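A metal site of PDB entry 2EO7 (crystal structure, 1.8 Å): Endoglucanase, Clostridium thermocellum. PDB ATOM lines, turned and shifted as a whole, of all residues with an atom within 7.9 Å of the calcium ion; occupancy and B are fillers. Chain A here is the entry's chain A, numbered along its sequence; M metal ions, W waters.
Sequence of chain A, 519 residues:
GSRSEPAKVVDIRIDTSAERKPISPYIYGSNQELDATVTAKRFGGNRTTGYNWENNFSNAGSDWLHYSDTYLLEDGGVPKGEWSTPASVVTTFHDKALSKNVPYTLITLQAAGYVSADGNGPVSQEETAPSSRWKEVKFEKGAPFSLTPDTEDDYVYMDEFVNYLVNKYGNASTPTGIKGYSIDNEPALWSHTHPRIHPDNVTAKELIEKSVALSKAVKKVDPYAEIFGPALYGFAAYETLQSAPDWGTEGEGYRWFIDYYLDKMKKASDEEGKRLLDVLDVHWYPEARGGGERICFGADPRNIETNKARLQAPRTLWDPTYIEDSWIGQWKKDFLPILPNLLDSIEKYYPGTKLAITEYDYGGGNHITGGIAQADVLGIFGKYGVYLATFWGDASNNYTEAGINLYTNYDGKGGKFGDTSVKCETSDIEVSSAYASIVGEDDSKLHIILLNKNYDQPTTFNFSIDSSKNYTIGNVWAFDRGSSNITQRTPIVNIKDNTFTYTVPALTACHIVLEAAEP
The backbone NH of Glu 54 lies close to the side-chain amide nitrogen of Asn 52.
The side-chain amino group of Lys 135 is in hydrogen-bond range of the backbone carbonyl oxygen of Asp 153 (2.9 Å).
The side-chain carboxylate (OD1) of Asp 150 sits at hydrogen-bond distance from the backbone NH (N) of Glu 152, at 2.8 Å.
Within 4 Å of the calcium ion: Glu 54, Asp 150, Asp 153 and Tyr 155.
Along chain A the residues within 4 Å of the calcium ion span positions 54 to 155.
The nearest printed residue that does not touch the calcium ion is Thr 151 (4.3 Å).
The calcium ion is bound by O of Asp 150 (2.2 Å).
The calcium ion is bound by O of Tyr 155.
Water W1 binds the calcium ion (2.4 Å).
The calcium ion is bound by OD1 of Asp 153 (2.4 Å).
The calcium ion is bound by OE1 of Glu 54 (2.4 Å).
The calcium ion is bound by water W2, 2.5 Å away.
The calcium ion is bound by OE2 of Glu 54 (2.5 Å).
The calcium ion has seven donor atoms within binding distance.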
ATOM      1  N   ASN A  52       6.629  -9.116  -3.697  1.00  0.00           N
ATOM      2  CA  ASN A  52       5.213  -8.977  -4.048  1.00  0.00           C
ATOM      3  C   ASN A  52       4.392  -9.178  -2.775  1.00  0.00           C
ATOM      4  O   ASN A  52       4.278 -10.292  -2.291  1.00  0.00           O
ATOM      5  CB  ASN A  52       4.872 -10.043  -5.102  1.00  0.00           C
ATOM      6  CG  ASN A  52       3.444  -9.946  -5.615  1.00  0.00           C
ATOM      7  OD1 ASN A  52       3.116 -10.503  -6.694  1.00  0.00           O
ATOM      8  ND2 ASN A  52       2.581  -9.275  -4.870  1.00  0.00           N
ATOM      9  N   TRP A  53       3.854  -8.089  -2.212  1.00  0.00           N
ATOM     10  CA  TRP A  53       3.091  -8.205  -0.966  1.00  0.00           C
ATOM     11  C   TRP A  53       1.858  -9.095  -1.069  1.00  0.00           C
ATOM     12  O   TRP A  53       1.395  -9.621  -0.042  1.00  0.00           O
ATOM     13  CB  TRP A  53       2.664  -6.817  -0.468  1.00  0.00           C
ATOM     14  CG  TRP A  53       1.450  -6.221  -1.181  1.00  0.00           C
ATOM     15  CD1 TRP A  53       1.409  -5.647  -2.405  1.00  0.00           C
ATOM     16  CD2 TRP A  53       0.118  -6.165  -0.655  1.00  0.00           C
ATOM     17  NE1 TRP A  53       0.125  -5.208  -2.695  1.00  0.00           N
ATOM     18  CE2 TRP A  53      -0.684  -5.515  -1.628  1.00  0.00           C
ATOM     19  CE3 TRP A  53      -0.475  -6.592   0.546  1.00  0.00           C
ATOM     20  CZ2 TRP A  53      -2.056  -5.289  -1.436  1.00  0.00           C
ATOM     21  CZ3 TRP A  53      -1.839  -6.355   0.736  1.00  0.00           C
ATOM     22  CH2 TRP A  53      -2.616  -5.717  -0.248  1.00  0.00           C
ATOM     23  N   GLU A  54       1.339  -9.271  -2.284  1.00  0.00           N
ATOM     24  CA  GLU A  54       0.144 -10.089  -2.463  1.00  0.00           C
ATOM     25  C   GLU A  54       0.384 -11.569  -2.177  1.00  0.00           C
ATOM     26  O   GLU A  54      -0.520 -12.249  -1.656  1.00  0.00           O
ATOM     27  CB  GLU A  54      -0.423  -9.938  -3.892  1.00  0.00           C
ATOM     28  CG  GLU A  54      -0.685  -8.481  -4.327  1.00  0.00           C
ATOM     29  CD  GLU A  54      -1.482  -8.389  -5.632  1.00  0.00           C
ATOM     30  OE1 GLU A  54      -1.443  -9.350  -6.425  1.00  0.00           O
ATOM     31  OE2 GLU A  54      -2.145  -7.351  -5.868  1.00  0.00           O
ATOM     32  N   ASN A  55       1.580 -12.072  -2.486  1.00  0.00           N
ATOM     33  CA  ASN A  55       1.876 -13.481  -2.262  1.00  0.00           C
ATOM     34  C   ASN A  55       3.219 -13.774  -1.569  1.00  0.00           C
ATOM     35  O   ASN A  55       3.579 -14.928  -1.398  1.00  0.00           O
ATOM     36  CB  ASN A  55       1.822 -14.245  -3.585  1.00  0.00           C
ATOM     37  CG  ASN A  55       2.705 -13.621  -4.633  1.00  0.00           C
ATOM     38  OD1 ASN A  55       3.767 -13.106  -4.313  1.00  0.00           O
ATOM     39  ND2 ASN A  55       2.279 -13.697  -5.896  1.00  0.00           N
ATOM     40  N   LYS A 135       4.606  -9.302 -12.164  1.00  0.00           N
ATOM     41  CA  LYS A 135       3.386  -8.511 -12.037  1.00  0.00           C
ATOM     42  C   LYS A 135       3.872  -7.070 -12.088  1.00  0.00           C
ATOM     43  O   LYS A 135       4.891  -6.740 -11.468  1.00  0.00           O
ATOM     44  CB  LYS A 135       2.684  -8.753 -10.694  1.00  0.00           C
ATOM     45  CG  LYS A 135       2.181 -10.162 -10.510  1.00  0.00           C
ATOM     46  CD  LYS A 135       1.198 -10.541 -11.633  1.00  0.00           C
ATOM     47  CE  LYS A 135       0.607 -11.935 -11.395  1.00  0.00           C
ATOM     48  NZ  LYS A 135      -0.296 -12.313 -12.518  1.00  0.00           N
ATOM     49  N   GLU A 136       3.166  -6.205 -12.806  1.00  0.00           N
ATOM     50  CA  GLU A 136       3.560  -4.797 -12.918  1.00  0.00           C
ATOM     51  C   GLU A 136       3.134  -4.019 -11.689  1.00  0.00           C
ATOM     52  O   GLU A 136       2.013  -4.159 -11.197  1.00  0.00           O
ATOM     53  CB  GLU A 136       2.912  -4.148 -14.156  1.00  0.00           C
ATOM     54  CG  GLU A 136       3.305  -2.680 -14.383  1.00  0.00           C
ATOM     55  CD  GLU A 136       2.650  -2.050 -15.607  1.00  0.00           C
ATOM     56  OE1 GLU A 136       2.386  -2.754 -16.596  1.00  0.00           O
ATOM     57  OE2 GLU A 136       2.409  -0.814 -15.595  1.00  0.00           O
ATOM     58  N   LYS A 141      -3.968   2.526  -7.079  1.00  0.00           N
ATOM     59  CA  LYS A 141      -4.955   1.606  -7.639  1.00  0.00           C
ATOM     60  C   LYS A 141      -6.042   2.340  -8.439  1.00  0.00           C
ATOM     61  O   LYS A 141      -6.435   1.886  -9.520  1.00  0.00           O
ATOM     62  CB  LYS A 141      -5.602   0.781  -6.513  1.00  0.00           C
ATOM     63  CG  LYS A 141      -6.462  -0.366  -7.040  1.00  0.00           C
ATOM     64  CD  LYS A 141      -7.075  -1.200  -5.916  1.00  0.00           C
ATOM     65  CE  LYS A 141      -7.746  -2.429  -6.494  1.00  0.00           C
ATOM     66  NZ  LYS A 141      -8.376  -3.273  -5.442  1.00  0.00           N
ATOM     67  N   PRO A 149      -6.214  -8.721  -1.805  1.00  0.00           N
ATOM     68  CA  PRO A 149      -5.806  -8.373  -3.163  1.00  0.00           C
ATOM     69  C   PRO A 149      -5.942  -9.522  -4.159  1.00  0.00           C
ATOM     70  O   PRO A 149      -5.767 -10.688  -3.821  1.00  0.00           O
ATOM     71  CB  PRO A 149      -4.364  -7.908  -2.980  1.00  0.00           C
ATOM     72  CG  PRO A 149      -3.885  -8.776  -1.856  1.00  0.00           C
ATOM     73  CD  PRO A 149      -5.058  -8.734  -0.891  1.00  0.00           C
ATOM     74  N   ASP A 150      -6.260  -9.161  -5.396  1.00  0.00           N
ATOM     75  CA  ASP A 150      -6.406 -10.151  -6.449  1.00  0.00           C
ATOM     76  C   ASP A 150      -5.035 -10.534  -6.973  1.00  0.00           C
ATOM     77  O   ASP A 150      -4.311  -9.703  -7.518  1.00  0.00           O
ATOM     78  CB  ASP A 150      -7.257  -9.565  -7.569  1.00  0.00           C
ATOM     79  CG  ASP A 150      -7.336 -10.482  -8.769  1.00  0.00           C
ATOM     80  OD1 ASP A 150      -7.095 -11.704  -8.628  1.00  0.00           O
ATOM     81  OD2 ASP A 150      -7.656  -9.985  -9.875  1.00  0.00           O
ATOM     82  N   THR A 151      -4.666 -11.805  -6.811  1.00  0.00           N
ATOM     83  CA  THR A 151      -3.374 -12.301  -7.255  1.00  0.00           C
ATOM     84  C   THR A 151      -3.418 -12.796  -8.685  1.00  0.00           C
ATOM     85  O   THR A 151      -2.390 -13.144  -9.264  1.00  0.00           O
ATOM     86  CB  THR A 151      -2.875 -13.455  -6.345  1.00  0.00           C
ATOM     87  OG1 THR A 151      -3.788 -14.562  -6.441  1.00  0.00           O
ATOM     88  CG2 THR A 151      -2.799 -13.000  -4.903  1.00  0.00           C
ATOM     89  N   GLU A 152      -4.613 -12.793  -9.270  1.00  0.00           N
ATOM     90  CA  GLU A 152      -4.786 -13.267 -10.636  1.00  0.00           C
ATOM     91  C   GLU A 152      -4.632 -12.197 -11.713  1.00  0.00           C
ATOM     92  O   GLU A 152      -4.404 -12.531 -12.883  1.00  0.00           O
ATOM     93  CB  GLU A 152      -6.148 -13.939 -10.776  1.00  0.00           C
ATOM     94  CG  GLU A 152      -6.388 -15.054  -9.762  1.00  0.00           C
ATOM     95  CD  GLU A 152      -5.319 -16.122  -9.822  1.00  0.00           C
ATOM     96  OE1 GLU A 152      -5.271 -16.855 -10.832  1.00  0.00           O
ATOM     97  OE2 GLU A 152      -4.524 -16.219  -8.860  1.00  0.00           O
ATOM     98  N   ASP A 153      -4.761 -10.921 -11.348  1.00  0.00           N
ATOM     99  CA  ASP A 153      -4.613  -9.888 -12.363  1.00  0.00           C
ATOM    100  C   ASP A 153      -3.138  -9.607 -12.602  1.00  0.00           C
ATOM    101  O   ASP A 153      -2.284 -10.277 -12.012  1.00  0.00           O
ATOM    102  CB  ASP A 153      -5.389  -8.614 -12.008  1.00  0.00           C
ATOM    103  CG  ASP A 153      -4.938  -7.982 -10.716  1.00  0.00           C
ATOM    104  OD1 ASP A 153      -3.845  -8.332 -10.226  1.00  0.00           O
ATOM    105  OD2 ASP A 153      -5.690  -7.134 -10.192  1.00  0.00           O
ATOM    106  N   ASP A 154      -2.831  -8.648 -13.472  1.00  0.00           N
ATOM    107  CA  ASP A 154      -1.439  -8.341 -13.812  1.00  0.00           C
ATOM    108  C   ASP A 154      -0.752  -7.248 -13.002  1.00  0.00           C
ATOM    109  O   ASP A 154       0.383  -6.883 -13.315  1.00  0.00           O
ATOM    110  CB  ASP A 154      -1.339  -7.934 -15.280  1.00  0.00           C
ATOM    111  CG  ASP A 154      -1.908  -8.981 -16.218  1.00  0.00           C
ATOM    112  OD1 ASP A 154      -1.753 -10.191 -15.940  1.00  0.00           O
ATOM    113  OD2 ASP A 154      -2.501  -8.581 -17.236  1.00  0.00           O
ATOM    114  N   TYR A 155      -1.415  -6.743 -11.965  1.00  0.00           N
ATOM    115  CA  TYR A 155      -0.847  -5.632 -11.206  1.00  0.00           C
ATOM    116  C   TYR A 155      -0.780  -5.801  -9.712  1.00  0.00           C
ATOM    117  O   TYR A 155      -1.524  -6.581  -9.123  1.00  0.00           O
ATOM    118  CB  TYR A 155      -1.665  -4.372 -11.474  1.00  0.00           C
ATOM    119  CG  TYR A 155      -1.761  -4.012 -12.933  1.00  0.00           C
ATOM    120  CD1 TYR A 155      -0.700  -3.370 -13.583  1.00  0.00           C
ATOM    121  CD2 TYR A 155      -2.889  -4.338 -13.682  1.00  0.00           C
ATOM    122  CE1 TYR A 155      -0.772  -3.059 -14.933  1.00  0.00           C
ATOM    123  CE2 TYR A 155      -2.970  -4.031 -15.042  1.00  0.00           C
ATOM    124  CZ  TYR A 155      -1.908  -3.390 -15.650  1.00  0.00           C
ATOM    125  OH  TYR A 155      -1.971  -3.076 -16.990  1.00  0.00           O
ATOM    126  N   VAL A 156       0.138  -5.062  -9.102  1.00  0.00           N
ATOM    127  CA  VAL A 156       0.302  -5.045  -7.659  1.00  0.00           C
ATOM    128  C   VAL A 156       0.341  -3.556  -7.345  1.00  0.00           C
ATOM    129  O   VAL A 156       1.118  -2.806  -7.959  1.00  0.00           O
ATOM    130  CB  VAL A 156       1.591  -5.756  -7.225  1.00  0.00           C
ATOM    131  CG1 VAL A 156       1.797  -5.573  -5.738  1.00  0.00           C
ATOM    132  CG2 VAL A 156       1.471  -7.262  -7.532  1.00  0.00           C
ATOM    133  N   TYR A 157      -0.511  -3.119  -6.424  1.00  0.00           N
ATOM    134  CA  TYR A 157      -0.653  -1.710  -6.073  1.00  0.00           C
ATOM    135  C   TYR A 157       0.012  -1.329  -4.767  1.00  0.00           C
ATOM    136  O   TYR A 157      -0.241  -1.933  -3.731  1.00  0.00           O
ATOM    137  CB  TYR A 157      -2.147  -1.380  -6.011  1.00  0.00           C
ATOM    138  CG  TYR A 157      -2.867  -1.707  -7.301  1.00  0.00           C
ATOM    139  CD1 TYR A 157      -2.744  -0.854  -8.405  1.00  0.00           C
ATOM    140  CD2 TYR A 157      -3.637  -2.862  -7.445  1.00  0.00           C
ATOM    141  CE1 TYR A 157      -3.360  -1.153  -9.612  1.00  0.00           C
ATOM    142  CE2 TYR A 157      -4.265  -3.172  -8.667  1.00  0.00           C
ATOM    143  CZ  TYR A 157      -4.124  -2.299  -9.734  1.00  0.00           C
ATOM    144  OH  TYR A 157      -4.717  -2.572 -10.954  1.00  0.00           O
ATOM    145  N   GLU A 160      -2.432   0.112  -2.049  1.00  0.00           N
ATOM    146  CA  GLU A 160      -3.289  -0.918  -1.474  1.00  0.00           C
ATOM    147  C   GLU A 160      -2.483  -1.678  -0.403  1.00  0.00           C
ATOM    148  O   GLU A 160      -3.029  -2.115   0.616  1.00  0.00           O
ATOM    149  CB  GLU A 160      -3.781  -1.850  -2.575  1.00  0.00           C
ATOM    150  CG  GLU A 160      -4.800  -2.877  -2.106  1.00  0.00           C
ATOM    151  CD  GLU A 160      -5.463  -3.608  -3.259  1.00  0.00           C
ATOM    152  OE1 GLU A 160      -4.735  -4.244  -4.075  1.00  0.00           O
ATOM    153  OE2 GLU A 160      -6.709  -3.529  -3.356  1.00  0.00           O
HETATM  154 CA    CA M   1      -2.771  -8.177  -8.098  1.00  0.00          CA
HETATM  155  O   HOH W   1      -1.502  -9.731  -9.382  1.00  0.00           O
HETATM  156  O   HOH W   2      -4.540  -6.489  -7.854  1.00  0.00           O
